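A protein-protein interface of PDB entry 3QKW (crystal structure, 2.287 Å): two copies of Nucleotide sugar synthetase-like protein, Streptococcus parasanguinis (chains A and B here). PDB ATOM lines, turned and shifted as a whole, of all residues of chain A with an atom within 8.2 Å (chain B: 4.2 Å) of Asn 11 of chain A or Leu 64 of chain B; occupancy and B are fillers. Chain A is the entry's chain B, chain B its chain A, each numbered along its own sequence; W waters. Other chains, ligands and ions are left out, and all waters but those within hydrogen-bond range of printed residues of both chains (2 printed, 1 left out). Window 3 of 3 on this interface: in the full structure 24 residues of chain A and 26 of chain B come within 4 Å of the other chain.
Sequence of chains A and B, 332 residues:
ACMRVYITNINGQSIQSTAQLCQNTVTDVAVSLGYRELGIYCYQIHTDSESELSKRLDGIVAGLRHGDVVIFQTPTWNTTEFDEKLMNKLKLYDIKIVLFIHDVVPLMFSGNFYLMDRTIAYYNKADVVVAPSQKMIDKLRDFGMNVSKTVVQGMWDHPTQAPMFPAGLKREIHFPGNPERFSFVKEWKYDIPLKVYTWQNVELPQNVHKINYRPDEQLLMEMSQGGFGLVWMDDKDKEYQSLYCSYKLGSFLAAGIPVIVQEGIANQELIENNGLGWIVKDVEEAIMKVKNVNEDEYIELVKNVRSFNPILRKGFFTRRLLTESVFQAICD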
ATOM      1  N   THR A   8       5.218  28.690  -9.898  1.00  0.00           N
ATOM      2  CA  THR A   8       5.255  28.060 -11.210  1.00  0.00           C
ATOM      3  C   THR A   8       3.886  28.192 -11.858  1.00  0.00           C
ATOM      4  O   THR A   8       2.860  28.210 -11.178  1.00  0.00           O
ATOM      5  CB  THR A   8       5.684  26.584 -11.143  1.00  0.00           C
ATOM      6  OG1 THR A   8       4.659  25.788 -10.540  1.00  0.00           O
ATOM      7  CG2 THR A   8       6.961  26.451 -10.306  1.00  0.00           C
ATOM      8  N   ASN A   9       3.885  28.294 -13.177  1.00  0.00           N
ATOM      9  CA  ASN A   9       2.654  28.442 -13.926  1.00  0.00           C
ATOM     10  C   ASN A   9       2.732  27.798 -15.319  1.00  0.00           C
ATOM     11  O   ASN A   9       3.518  28.235 -16.152  1.00  0.00           O
ATOM     12  CB  ASN A   9       2.397  29.927 -14.103  1.00  0.00           C
ATOM     13  CG  ASN A   9       1.034  30.213 -14.658  1.00  0.00           C
ATOM     14  OD1 ASN A   9       0.091  29.457 -14.427  1.00  0.00           O
ATOM     15  ND2 ASN A   9       0.915  31.314 -15.395  1.00  0.00           N
ATOM     16  N   ILE A  10       1.923  26.778 -15.587  1.00  0.00           N
ATOM     17  CA  ILE A  10       1.974  26.160 -16.911  1.00  0.00           C
ATOM     18  C   ILE A  10       1.352  27.034 -17.993  1.00  0.00           C
ATOM     19  O   ILE A  10       0.502  27.897 -17.740  1.00  0.00           O
ATOM     20  CB  ILE A  10       1.372  24.755 -16.948  1.00  0.00           C
ATOM     21  CG1 ILE A  10      -0.107  24.788 -16.573  1.00  0.00           C
ATOM     22  CG2 ILE A  10       2.131  23.853 -16.007  1.00  0.00           C
ATOM     23  CD1 ILE A  10      -0.849  23.509 -16.881  1.00  0.00           C
ATOM     24  N   ASN A  11       1.818  26.798 -19.208  1.00  0.00           N
ATOM     25  CA  ASN A  11       1.409  27.539 -20.384  1.00  0.00           C
ATOM     26  C   ASN A  11       1.461  26.560 -21.555  1.00  0.00           C
ATOM     27  O   ASN A  11       2.134  25.523 -21.464  1.00  0.00           O
ATOM     28  CB  ASN A  11       2.369  28.703 -20.585  1.00  0.00           C
ATOM     29  CG  ASN A  11       2.108  29.465 -21.842  1.00  0.00           C
ATOM     30  OD1 ASN A  11       3.022  30.075 -22.427  1.00  0.00           O
ATOM     31  ND2 ASN A  11       0.858  29.446 -22.281  1.00  0.00           N
ATOM     32  N   GLY A  12       0.740  26.863 -22.631  1.00  0.00           N
ATOM     33  CA  GLY A  12       0.797  26.057 -23.844  1.00  0.00           C
ATOM     34  C   GLY A  12      -0.164  24.876 -23.913  1.00  0.00           C
ATOM     35  O   GLY A  12      -0.042  24.026 -24.779  1.00  0.00           O
ATOM     36  N   GLN A  13      -1.114  24.779 -22.994  1.00  0.00           N
ATOM     37  CA  GLN A  13      -2.165  23.789 -23.188  1.00  0.00           C
ATOM     38  C   GLN A  13      -3.360  24.379 -23.930  1.00  0.00           C
ATOM     39  O   GLN A  13      -3.427  25.592 -24.181  1.00  0.00           O
ATOM     40  CB  GLN A  13      -2.577  23.111 -21.887  1.00  0.00           C
ATOM     41  CG  GLN A  13      -1.451  22.301 -21.268  1.00  0.00           C
ATOM     42  CD  GLN A  13      -1.948  21.214 -20.336  1.00  0.00           C
ATOM     43  OE1 GLN A  13      -2.468  21.495 -19.254  1.00  0.00           O
ATOM     44  NE2 GLN A  13      -1.791  19.956 -20.752  1.00  0.00           N
ATOM     45  N   SER A  14      -4.277  23.498 -24.314  1.00  0.00           N
ATOM     46  CA  SER A  14      -5.464  23.886 -25.060  1.00  0.00           C
ATOM     47  C   SER A  14      -6.354  24.800 -24.245  1.00  0.00           C
ATOM     48  O   SER A  14      -6.368  24.751 -23.011  1.00  0.00           O
ATOM     49  CB  SER A  14      -6.264  22.652 -25.450  1.00  0.00           C
ATOM     50  OG  SER A  14      -7.645  22.946 -25.408  1.00  0.00           O
ATOM     51  N   ALA A  19      -6.789  22.381 -15.943  1.00  0.00           N
ATOM     52  CA  ALA A  19      -5.512  22.455 -15.244  1.00  0.00           C
ATOM     53  C   ALA A  19      -4.823  23.794 -15.490  1.00  0.00           C
ATOM     54  O   ALA A  19      -4.347  24.426 -14.550  1.00  0.00           O
ATOM     55  CB  ALA A  19      -4.573  21.281 -15.640  1.00  0.00           C
ATOM     56  N   GLN A  20      -4.759  24.227 -16.746  1.00  0.00           N
ATOM     57  CA  GLN A  20      -4.072  25.480 -17.058  1.00  0.00           C
ATOM     58  C   GLN A  20      -4.834  26.687 -16.527  1.00  0.00           C
ATOM     59  O   GLN A  20      -4.262  27.583 -15.895  1.00  0.00           O
ATOM     60  CB  GLN A  20      -3.852  25.636 -18.555  1.00  0.00           C
ATOM     61  CG  GLN A  20      -3.314  27.005 -18.912  1.00  0.00           C
ATOM     62  CD  GLN A  20      -2.584  27.015 -20.244  1.00  0.00           C
ATOM     63  OE1 GLN A  20      -2.311  28.070 -20.810  1.00  0.00           O
ATOM     64  NE2 GLN A  20      -2.248  25.842 -20.737  1.00  0.00           N
ATOM     65  N   GLN A  23      -4.115  27.000 -12.944  1.00  0.00           N
ATOM     66  CA  GLN A  23      -2.769  27.433 -12.590  1.00  0.00           C
ATOM     67  C   GLN A  23      -2.641  28.912 -12.923  1.00  0.00           C
ATOM     68  O   GLN A  23      -2.044  29.678 -12.168  1.00  0.00           O
ATOM     69  CB  GLN A  23      -1.685  26.584 -13.285  1.00  0.00           C
ATOM     70  CG  GLN A  23      -1.614  25.132 -12.786  1.00  0.00           C
ATOM     71  CD  GLN A  23      -0.214  24.514 -12.936  1.00  0.00           C
ATOM     72  OE1 GLN A  23       0.754  25.211 -13.205  1.00  0.00           O
ATOM     73  NE2 GLN A  23      -0.119  23.200 -12.765  1.00  0.00           N
ATOM     74  N   ASN A  24      -3.260  29.305 -14.036  1.00  0.00           N
ATOM     75  CA  ASN A  24      -3.212  30.683 -14.517  1.00  0.00           C
ATOM     76  C   ASN A  24      -4.003  31.633 -13.625  1.00  0.00           C
ATOM     77  O   ASN A  24      -3.587  32.775 -13.405  1.00  0.00           O
ATOM     78  CB  ASN A  24      -3.767  30.778 -15.940  1.00  0.00           C
ATOM     79  CG  ASN A  24      -2.880  30.118 -16.953  1.00  0.00           C
ATOM     80  OD1 ASN A  24      -3.269  29.921 -18.108  1.00  0.00           O
ATOM     81  ND2 ASN A  24      -1.681  29.763 -16.532  1.00  0.00           N
ATOM     82  N   GLU A  37       6.108  35.011 -11.502  1.00  0.00           N
ATOM     83  CA  GLU A  37       5.863  33.782 -12.249  1.00  0.00           C
ATOM     84  C   GLU A  37       7.144  33.040 -12.643  1.00  0.00           C
ATOM     85  O   GLU A  37       8.066  33.650 -13.147  1.00  0.00           O
ATOM     86  CB  GLU A  37       5.118  34.108 -13.526  1.00  0.00           C
ATOM     87  CG  GLU A  37       5.000  32.932 -14.471  1.00  0.00           C
ATOM     88  CD  GLU A  37       4.439  33.344 -15.810  1.00  0.00           C
ATOM     89  OE1 GLU A  37       3.215  33.202 -16.009  1.00  0.00           O
ATOM     90  OE2 GLU A  37       5.211  33.854 -16.647  1.00  0.00           O
ATOM     91  N   LEU A  38       7.176  31.730 -12.404  1.00  0.00           N
ATOM     92  CA  LEU A  38       8.109  30.818 -13.083  1.00  0.00           C
ATOM     93  C   LEU A  38       7.343  30.067 -14.191  1.00  0.00           C
ATOM     94  O   LEU A  38       6.754  29.016 -13.946  1.00  0.00           O
ATOM     95  CB  LEU A  38       8.705  29.812 -12.103  1.00  0.00           C
ATOM     96  CG  LEU A  38       9.653  30.375 -11.035  1.00  0.00           C
ATOM     97  CD1 LEU A  38      10.135  29.253 -10.155  1.00  0.00           C
ATOM     98  CD2 LEU A  38      10.842  31.086 -11.669  1.00  0.00           C
ATOM     99  N   GLY A  39       7.323  30.626 -15.395  1.00  0.00           N
ATOM    100  CA  GLY A  39       6.550  30.039 -16.482  1.00  0.00           C
ATOM    101  C   GLY A  39       7.128  28.713 -16.932  1.00  0.00           C
ATOM    102  O   GLY A  39       8.348  28.600 -17.155  1.00  0.00           O
ATOM    103  N   ILE A  40       6.257  27.711 -17.025  1.00  0.00           N
ATOM    104  CA  ILE A  40       6.619  26.392 -17.526  1.00  0.00           C
ATOM    105  C   ILE A  40       5.782  26.091 -18.764  1.00  0.00           C
ATOM    106  O   ILE A  40       4.574  26.310 -18.766  1.00  0.00           O
ATOM    107  CB  ILE A  40       6.357  25.306 -16.473  1.00  0.00           C
ATOM    108  CG1 ILE A  40       7.266  25.507 -15.259  1.00  0.00           C
ATOM    109  CG2 ILE A  40       6.627  23.922 -17.053  1.00  0.00           C
ATOM    110  CD1 ILE A  40       6.777  24.775 -14.019  1.00  0.00           C
ATOM    111  N   TYR A  41       6.422  25.614 -19.826  1.00  0.00           N
ATOM    112  CA  TYR A  41       5.686  25.245 -21.035  1.00  0.00           C
ATOM    113  C   TYR A  41       5.452  23.731 -21.088  1.00  0.00           C
ATOM    114  O   TYR A  41       6.316  22.943 -20.694  1.00  0.00           O
ATOM    115  CB  TYR A  41       6.406  25.723 -22.300  1.00  0.00           C
ATOM    116  CG  TYR A  41       5.468  25.892 -23.468  1.00  0.00           C
ATOM    117  CD1 TYR A  41       4.869  27.120 -23.721  1.00  0.00           C
ATOM    118  CD2 TYR A  41       5.162  24.824 -24.310  1.00  0.00           C
ATOM    119  CE1 TYR A  41       4.008  27.288 -24.763  1.00  0.00           C
ATOM    120  CE2 TYR A  41       4.281  24.984 -25.375  1.00  0.00           C
ATOM    121  CZ  TYR A  41       3.705  26.230 -25.591  1.00  0.00           C
ATOM    122  OH  TYR A  41       2.820  26.447 -26.627  1.00  0.00           O
ATOM    123  N   CYS A  42       4.269  23.329 -21.539  1.00  0.00           N
ATOM    124  CA  CYS A  42       3.930  21.912 -21.628  1.00  0.00           C
ATOM    125  C   CYS A  42       4.364  21.345 -22.972  1.00  0.00           C
ATOM    126  O   CYS A  42       3.815  21.697 -24.010  1.00  0.00           O
ATOM    127  CB  CYS A  42       2.433  21.688 -21.391  1.00  0.00           C
ATOM    128  SG  CYS A  42       1.869  22.074 -19.680  1.00  0.00           S
ATOM    129  N   TYR A  43       5.369  20.477 -22.937  1.00  0.00           N
ATOM    130  CA  TYR A  43       5.871  19.832 -24.143  1.00  0.00           C
ATOM    131  C   TYR A  43       6.112  18.330 -23.914  1.00  0.00           C
ATOM    132  O   TYR A  43       5.710  17.779 -22.892  1.00  0.00           O
ATOM    133  CB  TYR A  43       7.157  20.520 -24.598  1.00  0.00           C
ATOM    134  CG  TYR A  43       8.331  20.287 -23.671  1.00  0.00           C
ATOM    135  CD1 TYR A  43       8.351  20.825 -22.373  1.00  0.00           C
ATOM    136  CD2 TYR A  43       9.433  19.543 -24.095  1.00  0.00           C
ATOM    137  CE1 TYR A  43       9.447  20.607 -21.522  1.00  0.00           C
ATOM    138  CE2 TYR A  43      10.534  19.316 -23.255  1.00  0.00           C
ATOM    139  CZ  TYR A  43      10.535  19.843 -21.975  1.00  0.00           C
ATOM    140  OH  TYR A  43      11.617  19.622 -21.167  1.00  0.00           O
ATOM    141  N   THR A  76       2.981  19.436 -13.277  1.00  0.00           N
ATOM    142  CA  THR A  76       3.185  20.315 -14.427  1.00  0.00           C
ATOM    143  C   THR A  76       2.478  19.788 -15.688  1.00  0.00           C
ATOM    144  O   THR A  76       2.261  20.535 -16.636  1.00  0.00           O
ATOM    145  CB  THR A  76       4.673  20.528 -14.748  1.00  0.00           C
ATOM    146  OG1 THR A  76       5.257  19.298 -15.212  1.00  0.00           O
ATOM    147  CG2 THR A  76       5.441  21.054 -13.522  1.00  0.00           C
ATOM    148  N   ASN A  78       3.969  17.640 -17.533  1.00  0.00           N
ATOM    149  CA  ASN A  78       5.068  17.177 -18.375  1.00  0.00           C
ATOM    150  C   ASN A  78       5.501  15.800 -17.903  1.00  0.00           C
ATOM    151  O   ASN A  78       6.512  15.283 -18.344  1.00  0.00           O
ATOM    152  CB  ASN A  78       6.252  18.146 -18.346  1.00  0.00           C
ATOM    153  CG  ASN A  78       5.964  19.430 -19.081  1.00  0.00           C
ATOM    154  OD1 ASN A  78       5.267  19.432 -20.099  1.00  0.00           O
ATOM    155  ND2 ASN A  78       6.482  20.545 -18.558  1.00  0.00           N
ATOM    156  N   TYR B   6       5.946  41.612 -20.047  1.00  0.00           N
ATOM    157  CA  TYR B   6       7.071  40.942 -19.432  1.00  0.00           C
ATOM    158  C   TYR B   6       8.273  41.840 -19.574  1.00  0.00           C
ATOM    159  O   TYR B   6       8.309  42.679 -20.472  1.00  0.00           O
ATOM    160  CB  TYR B   6       7.326  39.601 -20.122  1.00  0.00           C
ATOM    161  CG  TYR B   6       6.437  38.455 -19.677  1.00  0.00           C
ATOM    162  CD1 TYR B   6       5.127  38.343 -20.135  1.00  0.00           C
ATOM    163  CD2 TYR B   6       6.926  37.459 -18.834  1.00  0.00           C
ATOM    164  CE1 TYR B   6       4.321  37.279 -19.754  1.00  0.00           C
ATOM    165  CE2 TYR B   6       6.130  36.397 -18.441  1.00  0.00           C
ATOM    166  CZ  TYR B   6       4.831  36.309 -18.911  1.00  0.00           C
ATOM    167  OH  TYR B   6       4.028  35.265 -18.517  1.00  0.00           O
ATOM    168  N   VAL B  61      11.443  31.924 -21.866  1.00  0.00           N
ATOM    169  CA  VAL B  61      10.239  32.526 -22.419  1.00  0.00           C
ATOM    170  C   VAL B  61       9.043  31.574 -22.387  1.00  0.00           C
ATOM    171  O   VAL B  61       8.032  31.814 -23.030  1.00  0.00           O
ATOM    172  CB  VAL B  61      10.495  33.025 -23.845  1.00  0.00           C
ATOM    173  CG1 VAL B  61      11.742  33.868 -23.848  1.00  0.00           C
ATOM    174  CG2 VAL B  61      10.655  31.851 -24.816  1.00  0.00           C
ATOM    175  N   ALA B  62       9.160  30.500 -21.616  1.00  0.00           N
ATOM    176  CA  ALA B  62       8.107  29.494 -21.559  1.00  0.00           C
ATOM    177  C   ALA B  62       6.721  30.077 -21.294  1.00  0.00           C
ATOM    178  O   ALA B  62       5.705  29.531 -21.751  1.00  0.00           O
ATOM    179  CB  ALA B  62       8.445  28.454 -20.504  1.00  0.00           C
ATOM    180  N   GLY B  63       6.675  31.169 -20.540  1.00  0.00           N
ATOM    181  CA  GLY B  63       5.401  31.736 -20.123  1.00  0.00           C
ATOM    182  C   GLY B  63       4.818  32.734 -21.106  1.00  0.00           C
ATOM    183  O   GLY B  63       3.676  33.142 -20.948  1.00  0.00           O
ATOM    184  N   LEU B  64       5.599  33.127 -22.115  1.00  0.00           N
ATOM    185  CA  LEU B  64       5.137  34.057 -23.145  1.00  0.00           C
ATOM    186  C   LEU B  64       3.956  33.551 -23.988  1.00  0.00           C
ATOM    187  O   LEU B  64       3.803  32.345 -24.212  1.00  0.00           O
ATOM    188  CB  LEU B  64       6.280  34.404 -24.082  1.00  0.00           C
ATOM    189  CG  LEU B  64       7.088  35.650 -23.776  1.00  0.00           C
ATOM    190  CD1 LEU B  64       7.866  36.030 -25.016  1.00  0.00           C
ATOM    191  CD2 LEU B  64       6.143  36.763 -23.388  1.00  0.00           C
ATOM    192  N   ARG B  65       3.135  34.487 -24.457  1.00  0.00           N
ATOM    193  CA  ARG B  65       2.024  34.180 -25.360  1.00  0.00           C
ATOM    194  C   ARG B  65       1.860  35.246 -26.413  1.00  0.00           C
ATOM    195  O   ARG B  65       2.169  36.416 -26.172  1.00  0.00           O
ATOM    196  CB  ARG B  65       0.713  34.130 -24.599  1.00  0.00           C
ATOM    197  CG  ARG B  65       0.608  33.007 -23.631  1.00  0.00           C
ATOM    198  CD  ARG B  65      -0.761  33.021 -23.000  1.00  0.00           C
ATOM    199  NE  ARG B  65      -0.954  31.851 -22.161  1.00  0.00           N
ATOM    200  CZ  ARG B  65      -1.913  31.735 -21.254  1.00  0.00           C
ATOM    201  NH1 ARG B  65      -2.771  32.730 -21.067  1.00  0.00           N
ATOM    202  NH2 ARG B  65      -2.014  30.620 -20.540  1.00  0.00           N
ATOM    203  N   ASP B  68       1.270  39.304 -26.006  1.00  0.00           N
ATOM    204  CA  ASP B  68       1.955  39.903 -24.864  1.00  0.00           C
ATOM    205  C   ASP B  68       2.853  41.032 -25.328  1.00  0.00           C
ATOM    206  O   ASP B  68       3.043  41.228 -26.520  1.00  0.00           O
ATOM    207  CB  ASP B  68       2.764  38.860 -24.088  1.00  0.00           C
ATOM    208  CG  ASP B  68       1.878  37.920 -23.285  1.00  0.00           C
ATOM    209  OD1 ASP B  68       0.705  38.278 -23.029  1.00  0.00           O
ATOM    210  OD2 ASP B  68       2.363  36.828 -22.907  1.00  0.00           O
ATOM    211  N   VAL B  70       6.777  42.533 -24.520  1.00  0.00           N
ATOM    212  CA  VAL B  70       8.031  42.167 -23.854  1.00  0.00           C
ATOM    213  C   VAL B  70       9.039  43.303 -23.871  1.00  0.00           C
ATOM    214  O   VAL B  70       9.354  43.845 -24.927  1.00  0.00           O
ATOM    215  CB  VAL B  70       8.678  40.937 -24.531  1.00  0.00           C
ATOM    216  CG1 VAL B  70      10.134  40.753 -24.067  1.00  0.00           C
ATOM    217  CG2 VAL B  70       7.831  39.699 -24.286  1.00  0.00           C
ATOM    218  N   LEU B  90      12.176  36.043 -29.519  1.00  0.00           N
ATOM    219  CA  LEU B  90      11.042  36.907 -29.202  1.00  0.00           C
ATOM    220  C   LEU B  90      10.223  37.162 -30.459  1.00  0.00           C
ATOM    221  O   LEU B  90       9.004  37.186 -30.416  1.00  0.00           O
ATOM    222  CB  LEU B  90      11.496  38.233 -28.567  1.00  0.00           C
ATOM    223  CG  LEU B  90      12.131  38.220 -27.167  1.00  0.00           C
ATOM    224  CD1 LEU B  90      12.624  39.601 -26.787  1.00  0.00           C
ATOM    225  CD2 LEU B  90      11.160  37.691 -26.115  1.00  0.00           C
ATOM    226  N   TYR B  93       7.248  35.104 -31.689  1.00  0.00           N
ATOM    227  CA  TYR B  93       5.937  35.300 -31.098  1.00  0.00           C
ATOM    228  C   TYR B  93       5.279  36.500 -31.731  1.00  0.00           C
ATOM    229  O   TYR B  93       5.949  37.407 -32.219  1.00  0.00           O
ATOM    230  CB  TYR B  93       6.030  35.552 -29.593  1.00  0.00           C
ATOM    231  CG  TYR B  93       6.491  34.378 -28.755  1.00  0.00           C
ATOM    232  CD1 TYR B  93       7.847  34.076 -28.631  1.00  0.00           C
ATOM    233  CD2 TYR B  93       5.574  33.592 -28.062  1.00  0.00           C
ATOM    234  CE1 TYR B  93       8.272  33.019 -27.866  1.00  0.00           C
ATOM    235  CE2 TYR B  93       5.993  32.537 -27.284  1.00  0.00           C
ATOM    236  CZ  TYR B  93       7.346  32.252 -27.188  1.00  0.00           C
ATOM    237  OH  TYR B  93       7.772  31.192 -26.407  1.00  0.00           O
ATOM    238  N   ILE B  95       4.202  39.303 -30.744  1.00  0.00           N
ATOM    239  CA  ILE B  95       4.217  40.248 -29.648  1.00  0.00           C
ATOM    240  C   ILE B  95       4.854  41.543 -30.076  1.00  0.00           C
ATOM    241  O   ILE B  95       5.529  41.598 -31.113  1.00  0.00           O
ATOM    242  CB  ILE B  95       5.005  39.701 -28.468  1.00  0.00           C
ATOM    243  CG1 ILE B  95       6.467  39.505 -28.866  1.00  0.00           C
ATOM    244  CG2 ILE B  95       4.358  38.411 -27.944  1.00  0.00           C
ATOM    245  CD1 ILE B  95       7.322  38.915 -27.760  1.00  0.00           C
HETATM  246  O   HOH W   1       1.879  32.766 -18.647  1.00  0.00           O
HETATM  247  O   HOH W   2       0.579  30.621 -18.994  1.00  0.00           O
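ND2 of Asn 11 of chain A sits close to NE of Arg 65 of chain B, 3.0 Å away. The side-chain hydroxyl of Tyr 6 of chain B lies within hydrogen-bond range of the side-chain carboxylate of Glu 37 of chain A (2.6 Å). The side-chain amide oxygen (OE1) of Gln 20 of chain A sits at hydrogen-bond distance from the guanidinium group (NH2) of Arg 65 of chain B (2.6 Å). The backbone carbonyl oxygen (O) of Ala 62 of chain B sits close to the side-chain amide oxygen (OD1) of Asn 11 of chain A, at 2.8 Å. The guanidinium group of Arg 65 of chain B sits at hydrogen-bond distance from the side-chain amide oxygen of Asn 24 of chain A (2.8 Å). OD1 of Asn 11 of chain A lies close to O of Leu 64 of chain B. O of Gly 63 of chain B sits close to OD1 of Asn 11 of chain A (3.5 Å).
The side-chain carboxylate (OD2) of Asp 68 of chain B is in hydrogen-bond range of the backbone NH (N) of Arg 65 of chain B. The side-chain amide oxygen of Asn 24 of chain A sits close to the backbone carbonyl oxygen of Gln 20 of chain A (3.4 Å). The side-chain amide nitrogen (NE2) of Gln 20 of chain A sits close to the backbone NH (N) of Gln 13 of chain A. The backbone NH of Ile 40 of chain A sits at hydrogen-bond distance from the backbone carbonyl oxygen of Asn 9 of chain A (2.9 Å). O of Ile 10 of chain A sits at hydrogen-bond distance from ND2 of Asn 24 of chain A, at 3.1 Å. ND2 of Asn 9 of chain A is in hydrogen-bond range of OE1 of Glu 37 of chain A (3.0 Å).
Ala 62 of chain B touches Gly 39 of chain A (CB to O, 3.4 Å). Ile 40 of chain A touches Ala 62 of chain B. CD1 of Tyr 41 of chain A touches O of Ala 62 of chain B, 3.2 Å away.
Printed residues of chain B within 4 Å of Asn 11 of chain A: Ala 62 (2.8 Å), Gly 63 (3.5 Å), Leu 64 (3.0 Å) and Arg 65 (3.0 Å). Printed residues of chain B within 4 Å of Asn 24 of chain A: Arg 65 (2.8 Å). Printed residues of chain B within 4 Å of Gly 39 of chain A: Ala 62 (3.4 Å). Printed residues of chain B within 4 Å of Ile 40 of chain A: Ala 62. Of the printed residues of chain A, Tyr 6 of chain B touches Glu 37 (2.6 Å). Of chain A, only Asn 11 comes within 4 Å of Gly 63 of chain B. Leu 64 of chain B touches just one residue of chain A: Asn 11. Of the printed residues of chain A, Arg 65 of chain B touches Asn 11, Gln 20 and Asn 24. The nearest printed residue of chain B that does not touch Asn 11 of chain A is Val 61 of chain B (5.3 Å).
Of the 20 printed residues of chain A, 7 touch a printed residue of chain B. Printed residues of chain A that touch a printed residue of chain B: Asn 11, Gln 20, Asn 24, Glu 37, Gly 39, Ile 40 and Tyr 41. Of the 11 printed residues of chain B, 5 touch a printed residue of chain A. Printed residues of chain B that touch a printed residue of chain A: Tyr 6, Ala 62, Gly 63, Leu 64 and Arg 65. Among the printed residues, no Asp or Glu carboxylate lies within 4 Å of a Lys or Arg side-chain nitrogen of the other chain.
No position is printed for both chains.
Water W1 lies within hydrogen-bond range of O of Gly 63 of chain B (2.9 Å), OE1 of Glu 37 of chain A (3.0 Å) and OH of Tyr 6 of chain B (3.3 Å). Water W2 lies within hydrogen-bond range of the backbone carbonyl oxygen (O) of Ile 10 of chain A (3.0 Å), the guanidinium group (NH2) of Arg 65 of chain B (3.0 Å) and the side-chain amide nitrogen (ND2) of Asn 24 of chain A (3.5 Å).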
